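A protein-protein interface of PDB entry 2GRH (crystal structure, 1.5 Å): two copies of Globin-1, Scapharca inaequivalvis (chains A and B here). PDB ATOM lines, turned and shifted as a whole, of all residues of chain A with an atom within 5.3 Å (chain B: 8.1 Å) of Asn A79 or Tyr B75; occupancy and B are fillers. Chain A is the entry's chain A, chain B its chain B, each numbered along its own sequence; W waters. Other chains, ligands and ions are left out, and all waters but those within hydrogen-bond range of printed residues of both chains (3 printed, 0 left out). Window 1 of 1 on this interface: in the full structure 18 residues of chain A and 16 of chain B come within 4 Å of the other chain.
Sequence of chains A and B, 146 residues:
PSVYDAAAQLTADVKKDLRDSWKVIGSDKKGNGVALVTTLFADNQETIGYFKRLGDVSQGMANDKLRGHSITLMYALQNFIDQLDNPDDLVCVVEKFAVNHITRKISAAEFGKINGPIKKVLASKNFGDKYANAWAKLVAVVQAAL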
ATOM      1  N   MET A  74      -0.810 -12.541  13.866  1.00  0.00           N
ATOM      2  CA  MET A  74      -1.344 -12.267  12.537  1.00  0.00           C
ATOM      3  C   MET A  74      -0.401 -12.729  11.424  1.00  0.00           C
ATOM      4  O   MET A  74      -0.844 -13.048  10.321  1.00  0.00           O
ATOM      5  CB  MET A  74      -1.669 -10.776  12.390  1.00  0.00           C
ATOM      6  CG  MET A  74      -2.832 -10.312  13.266  1.00  0.00           C
ATOM      7  SD  MET A  74      -4.397 -11.131  12.882  1.00  0.00           S
ATOM      8  CE  MET A  74      -4.982 -10.109  11.558  1.00  0.00           C
ATOM      9  N   TYR A  75       0.898 -12.771  11.706  1.00  0.00           N
ATOM     10  CA  TYR A  75       1.858 -13.241  10.714  1.00  0.00           C
ATOM     11  C   TYR A  75       1.846 -14.764  10.619  1.00  0.00           C
ATOM     12  O   TYR A  75       2.293 -15.330   9.625  1.00  0.00           O
ATOM     13  CB  TYR A  75       3.257 -12.716  11.032  1.00  0.00           C
ATOM     14  CG  TYR A  75       3.441 -11.305  10.534  1.00  0.00           C
ATOM     15  CD1 TYR A  75       3.688 -11.051   9.184  1.00  0.00           C
ATOM     16  CD2 TYR A  75       3.282 -10.220  11.390  1.00  0.00           C
ATOM     17  CE1 TYR A  75       3.766  -9.749   8.697  1.00  0.00           C
ATOM     18  CE2 TYR A  75       3.354  -8.916  10.916  1.00  0.00           C
ATOM     19  CZ  TYR A  75       3.595  -8.687   9.571  1.00  0.00           C
ATOM     20  OH  TYR A  75       3.650  -7.395   9.108  1.00  0.00           O
ATOM     21  N   ALA A  76       1.335 -15.429  11.654  1.00  0.00           N
ATOM     22  CA  ALA A  76       1.215 -16.880  11.609  1.00  0.00           C
ATOM     23  C   ALA A  76       0.058 -17.152  10.642  1.00  0.00           C
ATOM     24  O   ALA A  76       0.133 -18.051   9.811  1.00  0.00           O
ATOM     25  CB  ALA A  76       0.899 -17.439  12.988  1.00  0.00           C
ATOM     26  N   LEU A  77      -1.007 -16.357  10.743  1.00  0.00           N
ATOM     27  CA  LEU A  77      -2.140 -16.534   9.841  1.00  0.00           C
ATOM     28  C   LEU A  77      -1.716 -16.185   8.409  1.00  0.00           C
ATOM     29  O   LEU A  77      -2.125 -16.852   7.457  1.00  0.00           O
ATOM     30  CB  LEU A  77      -3.328 -15.670  10.289  1.00  0.00           C
ATOM     31  CG  LEU A  77      -3.920 -16.054  11.655  1.00  0.00           C
ATOM     32  CD1 LEU A  77      -5.131 -15.175  11.948  1.00  0.00           C
ATOM     33  CD2 LEU A  77      -4.317 -17.525  11.665  1.00  0.00           C
ATOM     34  N   GLN A  78      -0.890 -15.150   8.252  1.00  0.00           N
ATOM     35  CA  GLN A  78      -0.398 -14.772   6.924  1.00  0.00           C
ATOM     36  C   GLN A  78       0.344 -15.963   6.310  1.00  0.00           C
ATOM     37  O   GLN A  78       0.192 -16.275   5.125  1.00  0.00           O
ATOM     38  CB  GLN A  78       0.558 -13.584   7.032  1.00  0.00           C
ATOM     39  CG  GLN A  78       1.192 -13.187   5.714  1.00  0.00           C
ATOM     40  CD  GLN A  78       0.201 -12.557   4.776  1.00  0.00           C
ATOM     41  OE1 GLN A  78      -0.429 -11.556   5.111  1.00  0.00           O
ATOM     42  NE2 GLN A  78       0.049 -13.137   3.590  1.00  0.00           N
ATOM     43  N   ASN A  79       1.157 -16.610   7.139  1.00  0.00           N
ATOM     44  CA  ASN A  79       1.938 -17.782   6.765  1.00  0.00           C
ATOM     45  C   ASN A  79       0.994 -18.877   6.238  1.00  0.00           C
ATOM     46  O   ASN A  79       1.202 -19.410   5.148  1.00  0.00           O
ATOM     47  CB  ASN A  79       2.698 -18.262   8.013  1.00  0.00           C
ATOM     48  CG  ASN A  79       3.784 -19.284   7.710  1.00  0.00           C
ATOM     49  OD1 ASN A  79       3.764 -19.967   6.689  1.00  0.00           O
ATOM     50  ND2 ASN A  79       4.738 -19.403   8.632  1.00  0.00           N
ATOM     51  N   PHE A  80      -0.050 -19.198   6.999  1.00  0.00           N
ATOM     52  CA  PHE A  80      -0.998 -20.231   6.568  1.00  0.00           C
ATOM     53  C   PHE A  80      -1.607 -19.896   5.214  1.00  0.00           C
ATOM     54  O   PHE A  80      -1.670 -20.744   4.326  1.00  0.00           O
ATOM     55  CB  PHE A  80      -2.143 -20.403   7.572  1.00  0.00           C
ATOM     56  CG  PHE A  80      -1.714 -20.876   8.936  1.00  0.00           C
ATOM     57  CD1 PHE A  80      -0.535 -21.591   9.121  1.00  0.00           C
ATOM     58  CD2 PHE A  80      -2.525 -20.627  10.039  1.00  0.00           C
ATOM     59  CE1 PHE A  80      -0.170 -22.052  10.392  1.00  0.00           C
ATOM     60  CE2 PHE A  80      -2.176 -21.080  11.310  1.00  0.00           C
ATOM     61  CZ  PHE A  80      -0.997 -21.793  11.488  1.00  0.00           C
ATOM     62  N   ILE A  81      -2.058 -18.656   5.055  1.00  0.00           N
ATOM     63  CA  ILE A  81      -2.678 -18.248   3.801  1.00  0.00           C
ATOM     64  C   ILE A  81      -1.719 -18.402   2.628  1.00  0.00           C
ATOM     65  O   ILE A  81      -2.106 -18.893   1.570  1.00  0.00           O
ATOM     66  CB  ILE A  81      -3.182 -16.789   3.880  1.00  0.00           C
ATOM     67  CG1 ILE A  81      -4.318 -16.696   4.904  1.00  0.00           C
ATOM     68  CG2 ILE A  81      -3.653 -16.314   2.507  1.00  0.00           C
ATOM     69  CD1 ILE A  81      -5.556 -17.527   4.545  1.00  0.00           C
ATOM     70  N   ASP A  82      -0.466 -17.999   2.818  1.00  0.00           N
ATOM     71  CA  ASP A  82       0.530 -18.111   1.759  1.00  0.00           C
ATOM     72  C   ASP A  82       0.866 -19.562   1.389  1.00  0.00           C
ATOM     73  O   ASP A  82       1.364 -19.810   0.293  1.00  0.00           O
ATOM     74  CB  ASP A  82       1.823 -17.379   2.150  1.00  0.00           C
ATOM     75  CG  ASP A  82       1.671 -15.866   2.140  1.00  0.00           C
ATOM     76  OD1 ASP A  82       0.723 -15.355   1.513  1.00  0.00           O
ATOM     77  OD2 ASP A  82       2.516 -15.178   2.750  1.00  0.00           O
ATOM     78  N   GLN A  83       0.593 -20.513   2.285  1.00  0.00           N
ATOM     79  CA  GLN A  83       0.884 -21.924   2.005  1.00  0.00           C
ATOM     80  C   GLN A  83      -0.302 -22.711   1.454  1.00  0.00           C
ATOM     81  O   GLN A  83      -0.181 -23.908   1.208  1.00  0.00           O
ATOM     82  CB  GLN A  83       1.363 -22.663   3.261  1.00  0.00           C
ATOM     83  CG  GLN A  83       2.463 -21.997   4.053  1.00  0.00           C
ATOM     84  CD  GLN A  83       3.528 -21.377   3.186  1.00  0.00           C
ATOM     85  OE1 GLN A  83       3.972 -21.969   2.205  1.00  0.00           O
ATOM     86  NE2 GLN A  83       3.954 -20.172   3.553  1.00  0.00           N
ATOM     87  N   VAL A  93       4.159 -26.024   8.399  1.00  0.00           N
ATOM     88  CA  VAL A  93       4.129 -24.791   9.185  1.00  0.00           C
ATOM     89  C   VAL A  93       3.075 -24.926  10.289  1.00  0.00           C
ATOM     90  O   VAL A  93       3.243 -24.399  11.386  1.00  0.00           O
ATOM     91  CB  VAL A  93       3.839 -23.531   8.322  1.00  0.00           C
ATOM     92  CG1 VAL A  93       5.020 -23.250   7.405  1.00  0.00           C
ATOM     93  CG2 VAL A  93       2.570 -23.718   7.518  1.00  0.00           C
ATOM     94  N   PHE A  97       3.661 -24.492  14.525  1.00  0.00           N
ATOM     95  CA  PHE A  97       2.889 -23.707  15.482  1.00  0.00           C
ATOM     96  C   PHE A  97       2.132 -24.582  16.469  1.00  0.00           C
ATOM     97  O   PHE A  97       1.833 -24.158  17.591  1.00  0.00           O
ATOM     98  CB  PHE A  97       1.929 -22.769  14.747  1.00  0.00           C
ATOM     99  CG  PHE A  97       2.619 -21.601  14.101  1.00  0.00           C
ATOM    100  CD1 PHE A  97       3.254 -20.639  14.882  1.00  0.00           C
ATOM    101  CD2 PHE A  97       2.665 -21.481  12.718  1.00  0.00           C
ATOM    102  CE1 PHE A  97       3.934 -19.571  14.290  1.00  0.00           C
ATOM    103  CE2 PHE A  97       3.343 -20.414  12.118  1.00  0.00           C
ATOM    104  CZ  PHE A  97       3.976 -19.461  12.906  1.00  0.00           C
ATOM    105  N   TRP B  22      14.633  -7.021   0.470  1.00  0.00           N
ATOM    106  CA  TRP B  22      13.628  -7.961   0.965  1.00  0.00           C
ATOM    107  C   TRP B  22      12.607  -8.293  -0.122  1.00  0.00           C
ATOM    108  O   TRP B  22      12.049  -9.390  -0.147  1.00  0.00           O
ATOM    109  CB  TRP B  22      12.908  -7.407   2.195  1.00  0.00           C
ATOM    110  CG  TRP B  22      11.930  -8.399   2.770  1.00  0.00           C
ATOM    111  CD1 TRP B  22      10.570  -8.302   2.769  1.00  0.00           C
ATOM    112  CD2 TRP B  22      12.243  -9.653   3.387  1.00  0.00           C
ATOM    113  NE1 TRP B  22      10.012  -9.420   3.347  1.00  0.00           N
ATOM    114  CE2 TRP B  22      11.017 -10.265   3.736  1.00  0.00           C
ATOM    115  CE3 TRP B  22      13.441 -10.321   3.679  1.00  0.00           C
ATOM    116  CZ2 TRP B  22      10.952 -11.514   4.361  1.00  0.00           C
ATOM    117  CZ3 TRP B  22      13.378 -11.568   4.302  1.00  0.00           C
ATOM    118  CH2 TRP B  22      12.137 -12.149   4.637  1.00  0.00           C
ATOM    119  N   GLY B  26      12.730 -12.015   0.087  1.00  0.00           N
ATOM    120  CA  GLY B  26      11.506 -12.380   0.776  1.00  0.00           C
ATOM    121  C   GLY B  26      10.441 -12.940  -0.155  1.00  0.00           C
ATOM    122  O   GLY B  26       9.379 -13.372   0.303  1.00  0.00           O
ATOM    123  N   LYS B  29      10.240 -17.436   0.342  1.00  0.00           N
ATOM    124  CA  LYS B  29      10.518 -17.737   1.736  1.00  0.00           C
ATOM    125  C   LYS B  29      10.977 -19.158   1.996  1.00  0.00           C
ATOM    126  O   LYS B  29      11.842 -19.381   2.837  1.00  0.00           O
ATOM    127  CB  LYS B  29       9.298 -17.390   2.590  1.00  0.00           C
ATOM    128  CG  LYS B  29       8.995 -15.899   2.571  1.00  0.00           C
ATOM    129  CD  LYS B  29       7.820 -15.552   3.454  1.00  0.00           C
ATOM    130  CE  LYS B  29       7.657 -14.045   3.606  1.00  0.00           C
ATOM    131  NZ  LYS B  29       7.391 -13.370   2.310  1.00  0.00           N
ATOM    132  N   LYS B  30      10.418 -20.123   1.279  1.00  0.00           N
ATOM    133  CA  LYS B  30      10.836 -21.504   1.479  1.00  0.00           C
ATOM    134  C   LYS B  30      12.270 -21.709   0.994  1.00  0.00           C
ATOM    135  O   LYS B  30      13.121 -22.211   1.732  1.00  0.00           O
ATOM    136  CB  LYS B  30       9.890 -22.463   0.745  1.00  0.00           C
ATOM    137  CG  LYS B  30      10.318 -23.924   0.825  1.00  0.00           C
ATOM    138  CD  LYS B  30       9.232 -24.879   0.338  1.00  0.00           C
ATOM    139  CE  LYS B  30       8.794 -24.577  -1.085  1.00  0.00           C
ATOM    140  NZ  LYS B  30       7.865 -25.630  -1.602  1.00  0.00           N
ATOM    141  N   GLY B  33      14.705 -19.224   2.882  1.00  0.00           N
ATOM    142  CA  GLY B  33      14.705 -19.486   4.308  1.00  0.00           C
ATOM    143  C   GLY B  33      15.545 -20.718   4.597  1.00  0.00           C
ATOM    144  O   GLY B  33      16.360 -20.722   5.518  1.00  0.00           O
ATOM    145  N   ARG B  67      11.965 -27.334   7.316  1.00  0.00           N
ATOM    146  CA  ARG B  67      11.293 -26.517   6.316  1.00  0.00           C
ATOM    147  C   ARG B  67      10.283 -25.615   7.023  1.00  0.00           C
ATOM    148  O   ARG B  67      10.226 -24.418   6.739  1.00  0.00           O
ATOM    149  CB  ARG B  67      10.601 -27.417   5.295  1.00  0.00           C
ATOM    150  CG  ARG B  67      10.322 -26.709   3.987  1.00  0.00           C
ATOM    151  CD  ARG B  67       9.905 -27.682   2.888  1.00  0.00           C
ATOM    152  NE  ARG B  67       8.615 -28.316   3.152  1.00  0.00           N
ATOM    153  CZ  ARG B  67       8.456 -29.573   3.558  1.00  0.00           C
ATOM    154  NH1 ARG B  67       9.510 -30.359   3.753  1.00  0.00           N
ATOM    155  NH2 ARG B  67       7.235 -30.048   3.771  1.00  0.00           N
ATOM    156  N   GLY B  68       9.508 -26.176   7.954  1.00  0.00           N
ATOM    157  CA  GLY B  68       8.522 -25.384   8.674  1.00  0.00           C
ATOM    158  C   GLY B  68       9.170 -24.286   9.498  1.00  0.00           C
ATOM    159  O   GLY B  68       8.670 -23.167   9.570  1.00  0.00           O
ATOM    160  N   HIS B  69      10.290 -24.615  10.127  1.00  0.00           N
ATOM    161  CA  HIS B  69      11.026 -23.648  10.929  1.00  0.00           C
ATOM    162  C   HIS B  69      11.585 -22.532  10.045  1.00  0.00           C
ATOM    163  O   HIS B  69      11.473 -21.351  10.373  1.00  0.00           O
ATOM    164  CB  HIS B  69      12.190 -24.345  11.645  1.00  0.00           C
ATOM    165  CG  HIS B  69      13.199 -23.398  12.217  1.00  0.00           C
ATOM    166  ND1 HIS B  69      13.002 -22.782  13.427  1.00  0.00           N
ATOM    167  CD2 HIS B  69      14.370 -22.972  11.679  1.00  0.00           C
ATOM    168  CE1 HIS B  69      14.048 -21.995  13.600  1.00  0.00           C
ATOM    169  NE2 HIS B  69      14.905 -22.075  12.568  1.00  0.00           N
ATOM    170  N   SER B  70      12.187 -22.912   8.925  1.00  0.00           N
ATOM    171  CA  SER B  70      12.792 -21.940   8.020  1.00  0.00           C
ATOM    172  C   SER B  70      11.785 -20.982   7.392  1.00  0.00           C
ATOM    173  O   SER B  70      12.058 -19.787   7.255  1.00  0.00           O
ATOM    174  CB  SER B  70      13.577 -22.664   6.930  1.00  0.00           C
ATOM    175  OG  SER B  70      14.573 -23.498   7.506  1.00  0.00           O
ATOM    176  N   ILE B  71      10.632 -21.504   6.991  1.00  0.00           N
ATOM    177  CA  ILE B  71       9.610 -20.646   6.406  1.00  0.00           C
ATOM    178  C   ILE B  71       9.146 -19.653   7.470  1.00  0.00           C
ATOM    179  O   ILE B  71       9.020 -18.453   7.210  1.00  0.00           O
ATOM    180  CB  ILE B  71       8.404 -21.469   5.915  1.00  0.00           C
ATOM    181  CG1 ILE B  71       8.800 -22.271   4.674  1.00  0.00           C
ATOM    182  CG2 ILE B  71       7.229 -20.538   5.589  1.00  0.00           C
ATOM    183  CD1 ILE B  71       7.772 -23.307   4.257  1.00  0.00           C
ATOM    184  N   THR B  72       8.905 -20.148   8.677  1.00  0.00           N
ATOM    185  CA  THR B  72       8.449 -19.293   9.762  1.00  0.00           C
ATOM    186  C   THR B  72       9.471 -18.219  10.129  1.00  0.00           C
ATOM    187  O   THR B  72       9.106 -17.091  10.467  1.00  0.00           O
ATOM    188  CB  THR B  72       8.080 -20.145  10.982  1.00  0.00           C
ATOM    189  OG1 THR B  72       7.060 -21.077  10.598  1.00  0.00           O
ATOM    190  CG2 THR B  72       7.562 -19.275  12.110  1.00  0.00           C
ATOM    191  N   LEU B  73      10.753 -18.555  10.054  1.00  0.00           N
ATOM    192  CA  LEU B  73      11.788 -17.574  10.353  1.00  0.00           C
ATOM    193  C   LEU B  73      11.678 -16.400   9.367  1.00  0.00           C
ATOM    194  O   LEU B  73      11.857 -15.234   9.740  1.00  0.00           O
ATOM    195  CB  LEU B  73      13.170 -18.239  10.264  1.00  0.00           C
ATOM    196  CG  LEU B  73      14.403 -17.361  10.493  1.00  0.00           C
ATOM    197  CD1 LEU B  73      15.578 -18.234  10.924  1.00  0.00           C
ATOM    198  CD2 LEU B  73      14.736 -16.592   9.228  1.00  0.00           C
ATOM    199  N   MET B  74      11.364 -16.699   8.113  1.00  0.00           N
ATOM    200  CA  MET B  74      11.245 -15.644   7.112  1.00  0.00           C
ATOM    201  C   MET B  74      10.064 -14.720   7.400  1.00  0.00           C
ATOM    202  O   MET B  74      10.078 -13.555   7.001  1.00  0.00           O
ATOM    203  CB  MET B  74      11.135 -16.246   5.709  1.00  0.00           C
ATOM    204  CG  MET B  74      12.399 -16.981   5.262  1.00  0.00           C
ATOM    205  SD  MET B  74      13.849 -15.904   5.127  1.00  0.00           S
ATOM    206  CE  MET B  74      13.659 -15.310   3.460  1.00  0.00           C
ATOM    207  N   TYR B  75       9.044 -15.228   8.087  1.00  0.00           N
ATOM    208  CA  TYR B  75       7.902 -14.382   8.433  1.00  0.00           C
ATOM    209  C   TYR B  75       8.229 -13.477   9.618  1.00  0.00           C
ATOM    210  O   TYR B  75       7.572 -12.460   9.824  1.00  0.00           O
ATOM    211  CB  TYR B  75       6.653 -15.230   8.704  1.00  0.00           C
ATOM    212  CG  TYR B  75       5.972 -15.635   7.423  1.00  0.00           C
ATOM    213  CD1 TYR B  75       5.080 -14.774   6.779  1.00  0.00           C
ATOM    214  CD2 TYR B  75       6.278 -16.843   6.806  1.00  0.00           C
ATOM    215  CE1 TYR B  75       4.518 -15.111   5.551  1.00  0.00           C
ATOM    216  CE2 TYR B  75       5.727 -17.187   5.580  1.00  0.00           C
ATOM    217  CZ  TYR B  75       4.849 -16.318   4.960  1.00  0.00           C
ATOM    218  OH  TYR B  75       4.328 -16.660   3.737  1.00  0.00           O
ATOM    219  N   ALA B  76       9.242 -13.845  10.398  1.00  0.00           N
ATOM    220  CA  ALA B  76       9.661 -13.001  11.506  1.00  0.00           C
ATOM    221  C   ALA B  76      10.350 -11.810  10.841  1.00  0.00           C
ATOM    222  O   ALA B  76      10.178 -10.666  11.256  1.00  0.00           O
ATOM    223  CB  ALA B  76      10.643 -13.745  12.411  1.00  0.00           C
ATOM    224  N   LEU B  77      11.126 -12.078   9.794  1.00  0.00           N
ATOM    225  CA  LEU B  77      11.803 -11.000   9.082  1.00  0.00           C
ATOM    226  C   LEU B  77      10.769 -10.146   8.350  1.00  0.00           C
ATOM    227  O   LEU B  77      10.909  -8.928   8.280  1.00  0.00           O
ATOM    228  CB  LEU B  77      12.839 -11.563   8.103  1.00  0.00           C
ATOM    229  CG  LEU B  77      13.994 -12.320   8.775  1.00  0.00           C
ATOM    230  CD1 LEU B  77      14.951 -12.832   7.708  1.00  0.00           C
ATOM    231  CD2 LEU B  77      14.721 -11.410   9.754  1.00  0.00           C
ATOM    232  N   GLN B  78       9.730 -10.778   7.809  1.00  0.00           N
ATOM    233  CA  GLN B  78       8.678 -10.022   7.124  1.00  0.00           C
ATOM    234  C   GLN B  78       8.065  -9.035   8.117  1.00  0.00           C
ATOM    235  O   GLN B  78       7.815  -7.870   7.791  1.00  0.00           O
ATOM    236  CB  GLN B  78       7.586 -10.966   6.618  1.00  0.00           C
ATOM    237  CG  GLN B  78       6.448 -10.259   5.896  1.00  0.00           C
ATOM    238  CD  GLN B  78       6.876  -9.689   4.569  1.00  0.00           C
ATOM    239  OE1 GLN B  78       7.387 -10.412   3.710  1.00  0.00           O
ATOM    240  NE2 GLN B  78       6.665  -8.384   4.382  1.00  0.00           N
ATOM    241  N   ASN B  79       7.831  -9.526   9.328  1.00  0.00           N
ATOM    242  CA  ASN B  79       7.263  -8.756  10.431  1.00  0.00           C
ATOM    243  C   ASN B  79       8.144  -7.524  10.677  1.00  0.00           C
ATOM    244  O   ASN B  79       7.668  -6.387  10.676  1.00  0.00           O
ATOM    245  CB  ASN B  79       7.240  -9.652  11.676  1.00  0.00           C
ATOM    246  CG  ASN B  79       6.360  -9.115  12.786  1.00  0.00           C
ATOM    247  OD1 ASN B  79       6.084  -7.920  12.865  1.00  0.00           O
ATOM    248  ND2 ASN B  79       5.922 -10.009  13.668  1.00  0.00           N
ATOM    249  N   PHE B  80       9.437  -7.758  10.873  1.00  0.00           N
ATOM    250  CA  PHE B  80      10.376  -6.666  11.111  1.00  0.00           C
ATOM    251  C   PHE B  80      10.333  -5.610  10.012  1.00  0.00           C
ATOM    252  O   PHE B  80      10.258  -4.409  10.293  1.00  0.00           O
ATOM    253  CB  PHE B  80      11.812  -7.191  11.195  1.00  0.00           C
ATOM    254  CG  PHE B  80      12.096  -8.054  12.393  1.00  0.00           C
ATOM    255  CD1 PHE B  80      11.210  -8.129  13.462  1.00  0.00           C
ATOM    256  CD2 PHE B  80      13.284  -8.772  12.458  1.00  0.00           C
ATOM    257  CE1 PHE B  80      11.505  -8.904  14.579  1.00  0.00           C
ATOM    258  CE2 PHE B  80      13.591  -9.550  13.572  1.00  0.00           C
ATOM    259  CZ  PHE B  80      12.701  -9.615  14.632  1.00  0.00           C
ATOM    260  N   ILE B  81      10.408  -6.058   8.762  1.00  0.00           N
ATOM    261  CA  ILE B  81      10.403  -5.146   7.624  1.00  0.00           C
ATOM    262  C   ILE B  81       9.121  -4.325   7.576  1.00  0.00           C
ATOM    263  O   ILE B  81       9.153  -3.132   7.271  1.00  0.00           O
ATOM    264  CB  ILE B  81      10.578  -5.912   6.291  1.00  0.00           C
ATOM    265  CG1 ILE B  81      11.937  -6.624   6.271  1.00  0.00           C
ATOM    266  CG2 ILE B  81      10.463  -4.948   5.111  1.00  0.00           C
ATOM    267  CD1 ILE B  81      13.147  -5.687   6.296  1.00  0.00           C
ATOM    268  N   ASP B  82       7.993  -4.957   7.886  1.00  0.00           N
ATOM    269  CA  ASP B  82       6.717  -4.249   7.867  1.00  0.00           C
ATOM    270  C   ASP B  82       6.581  -3.201   8.973  1.00  0.00           C
ATOM    271  O   ASP B  82       5.774  -2.275   8.851  1.00  0.00           O
ATOM    272  CB  ASP B  82       5.553  -5.243   7.967  1.00  0.00           C
ATOM    273  CG  ASP B  82       5.378  -6.073   6.709  1.00  0.00           C
ATOM    274  OD1 ASP B  82       5.987  -5.733   5.675  1.00  0.00           O
ATOM    275  OD2 ASP B  82       4.615  -7.062   6.750  1.00  0.00           O
ATOM    276  N   GLN B  83       7.362  -3.333  10.044  1.00  0.00           N
ATOM    277  CA  GLN B  83       7.297  -2.390  11.168  1.00  0.00           C
ATOM    278  C   GLN B  83       8.365  -1.298  11.140  1.00  0.00           C
ATOM    279  O   GLN B  83       8.459  -0.512  12.081  1.00  0.00           O
ATOM    280  CB  GLN B  83       7.450  -3.118  12.510  1.00  0.00           C
ATOM    281  CG  GLN B  83       6.629  -4.372  12.691  1.00  0.00           C
ATOM    282  CD  GLN B  83       5.199  -4.210  12.245  1.00  0.00           C
ATOM    283  OE1 GLN B  83       4.566  -3.181  12.491  1.00  0.00           O
ATOM    284  NE2 GLN B  83       4.669  -5.240  11.597  1.00  0.00           N
ATOM    285  N   PHE B  97      10.472 -11.759  19.803  1.00  0.00           N
ATOM    286  CA  PHE B  97      11.374 -12.771  19.275  1.00  0.00           C
ATOM    287  C   PHE B  97      12.646 -12.902  20.099  1.00  0.00           C
ATOM    288  O   PHE B  97      13.274 -13.962  20.117  1.00  0.00           O
ATOM    289  CB  PHE B  97      11.698 -12.479  17.807  1.00  0.00           C
ATOM    290  CG  PHE B  97      10.565 -12.806  16.879  1.00  0.00           C
ATOM    291  CD1 PHE B  97      10.129 -14.119  16.742  1.00  0.00           C
ATOM    292  CD2 PHE B  97       9.900 -11.802  16.188  1.00  0.00           C
ATOM    293  CE1 PHE B  97       9.040 -14.430  15.934  1.00  0.00           C
ATOM    294  CE2 PHE B  97       8.810 -12.101  15.377  1.00  0.00           C
ATOM    295  CZ  PHE B  97       8.379 -13.416  15.250  1.00  0.00           C
HETATM  296  O   HOH W   1       1.588  -6.374   6.904  1.00  0.00           O
HETATM  297  O   HOH W   2       1.975  -4.982   9.787  1.00  0.00           O
HETATM  298  O   HOH W   3       5.541 -18.162   1.536  1.00  0.00           O
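The side-chain amide nitrogen (ND2) of Asn A79 is in hydrogen-bond range of the side-chain hydroxyl (OG1) of Thr B72 (3.5 Å). The side-chain carboxylate of Asp A82 lies within hydrogen-bond range of the side-chain hydroxyl of Tyr B75 (2.5 Å). The side-chain hydroxyl of Tyr A75 sits at hydrogen-bond distance from the side-chain carboxylate of Asp B82 (2.6 Å). The side-chain hydroxyl (OH) of Tyr A75 lies within hydrogen-bond range of the side-chain amide nitrogen (NE2) of Gln B83 (3.4 Å).
The side-chain amide nitrogen (NE2) of Gln A83 is in hydrogen-bond range of the side-chain amide oxygen (OD1) of Asn A79, at 3.1 Å. OD1 of Asn B79 lies within hydrogen-bond range of NE2 of Gln B83 (3.3 Å). The side-chain carboxylate of Asp B82 sits at hydrogen-bond distance from the side-chain amide nitrogen of Gln B78 (3.0 Å). The side-chain carboxylate (OD1) of Asp A82 lies within hydrogen-bond range of the side-chain amide nitrogen (NE2) of Gln A78 (3.1 Å). NE1 of Trp B22 is in hydrogen-bond range of OE1 of Gln B78 (2.8 Å). The side-chain amino group of Lys B29 is in hydrogen-bond range of the side-chain amide oxygen of Gln B78 (3.3 Å).
Tyr A75 touches Gln B78. Asn B79 touches Tyr A75 (ND2 to CD2, 3.5 Å). Gln A78 touches Tyr B75 (CG to CE1, 3.8 Å). Asn A79 touches Ile B71. CD2 of Tyr B75 touches ND2 of Asn A79, 3.5 Å away. Ile B71 touches Gln A83 (CG2 to NE2, 3.9 Å). Tyr B75 touches Gln A83. CG1 of Val A93 touches CG2 of Ile B71, at 3.9 Å. CG2 of Thr B72 touches CZ of Phe A97 (3.7 Å).
Of chain B, only Ile B71 (3.7 Å), Thr B72 (3.5 Å) and Tyr B75 (3.5 Å) come within 4 Å of Asn A79. Tyr B75 touches just these residues of chain A: Gln A78, Asn A79, Asp A82 and Gln A83. Of the printed residues of chain B, Gln A83 touches Ile B71 and Tyr B75. Printed residues of chain A within 4 Å of Gln B83: Tyr A75 (3.4 Å). Of the printed residues of chain A, Thr B72 touches Asn A79 and Phe A97. Lys B30 touches none of the printed residues of chain A. The nearest residue of chain B that does not touch Asn A79 is Gly B68 (5.5 Å). The nearest residue of chain A that does not touch Tyr B75 is Tyr A75 (4.02 Å). The nearest printed residue of chain B that does not touch Phe A97 is Gly B68 (6.5 Å).
Of the 23 printed residues of chain B, 7 touch a printed residue of chain A. Hydrophobic or aromatic side chains of chain B within 4 Å of the printed part of chain A: Ile B71 and Tyr B75. Printed residues of chain A that touch a printed residue of chain B: Tyr A75, Gln A78, Asn A79, Asp A82, Gln A83, Val A93 and Phe A97. Hydrophobic or aromatic side chains of chain A within 4 Å of the printed part of chain B: Tyr A75, Val A93 and Phe A97. Among the printed residues, 13 pairs touch across the chains.
Tyr A75 touches Gln B78, and with the chains exchanged Gln A78 touches Tyr B75. Tyr A75 touches Asn B79, and with the chains exchanged Asn A79 touches Tyr B75. Tyr A75 touches Asp B82, and with the chains exchanged Asp A82 touches Tyr B75. Tyr A75 touches Gln B83, and with the chains exchanged Gln A83 touches Tyr B75. Positions printed for both chains: 74, 75, 76, 77, 78, 79, 80, 81, 82, 83 and 97.
Water W3 bridges OH of Tyr B75 (2.9 Å) and NE2 of Gln A83 (3.3 Å). Water W2 bridges OH of Tyr A75 (3.0 Å) and NE2 of Gln B83 (3.3 Å). Water W1 bridges the side-chain carboxylate (OD2) of Asp B82 (3.1 Å) and the side-chain hydroxyl (OH) of Tyr A75 (3.2 Å).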
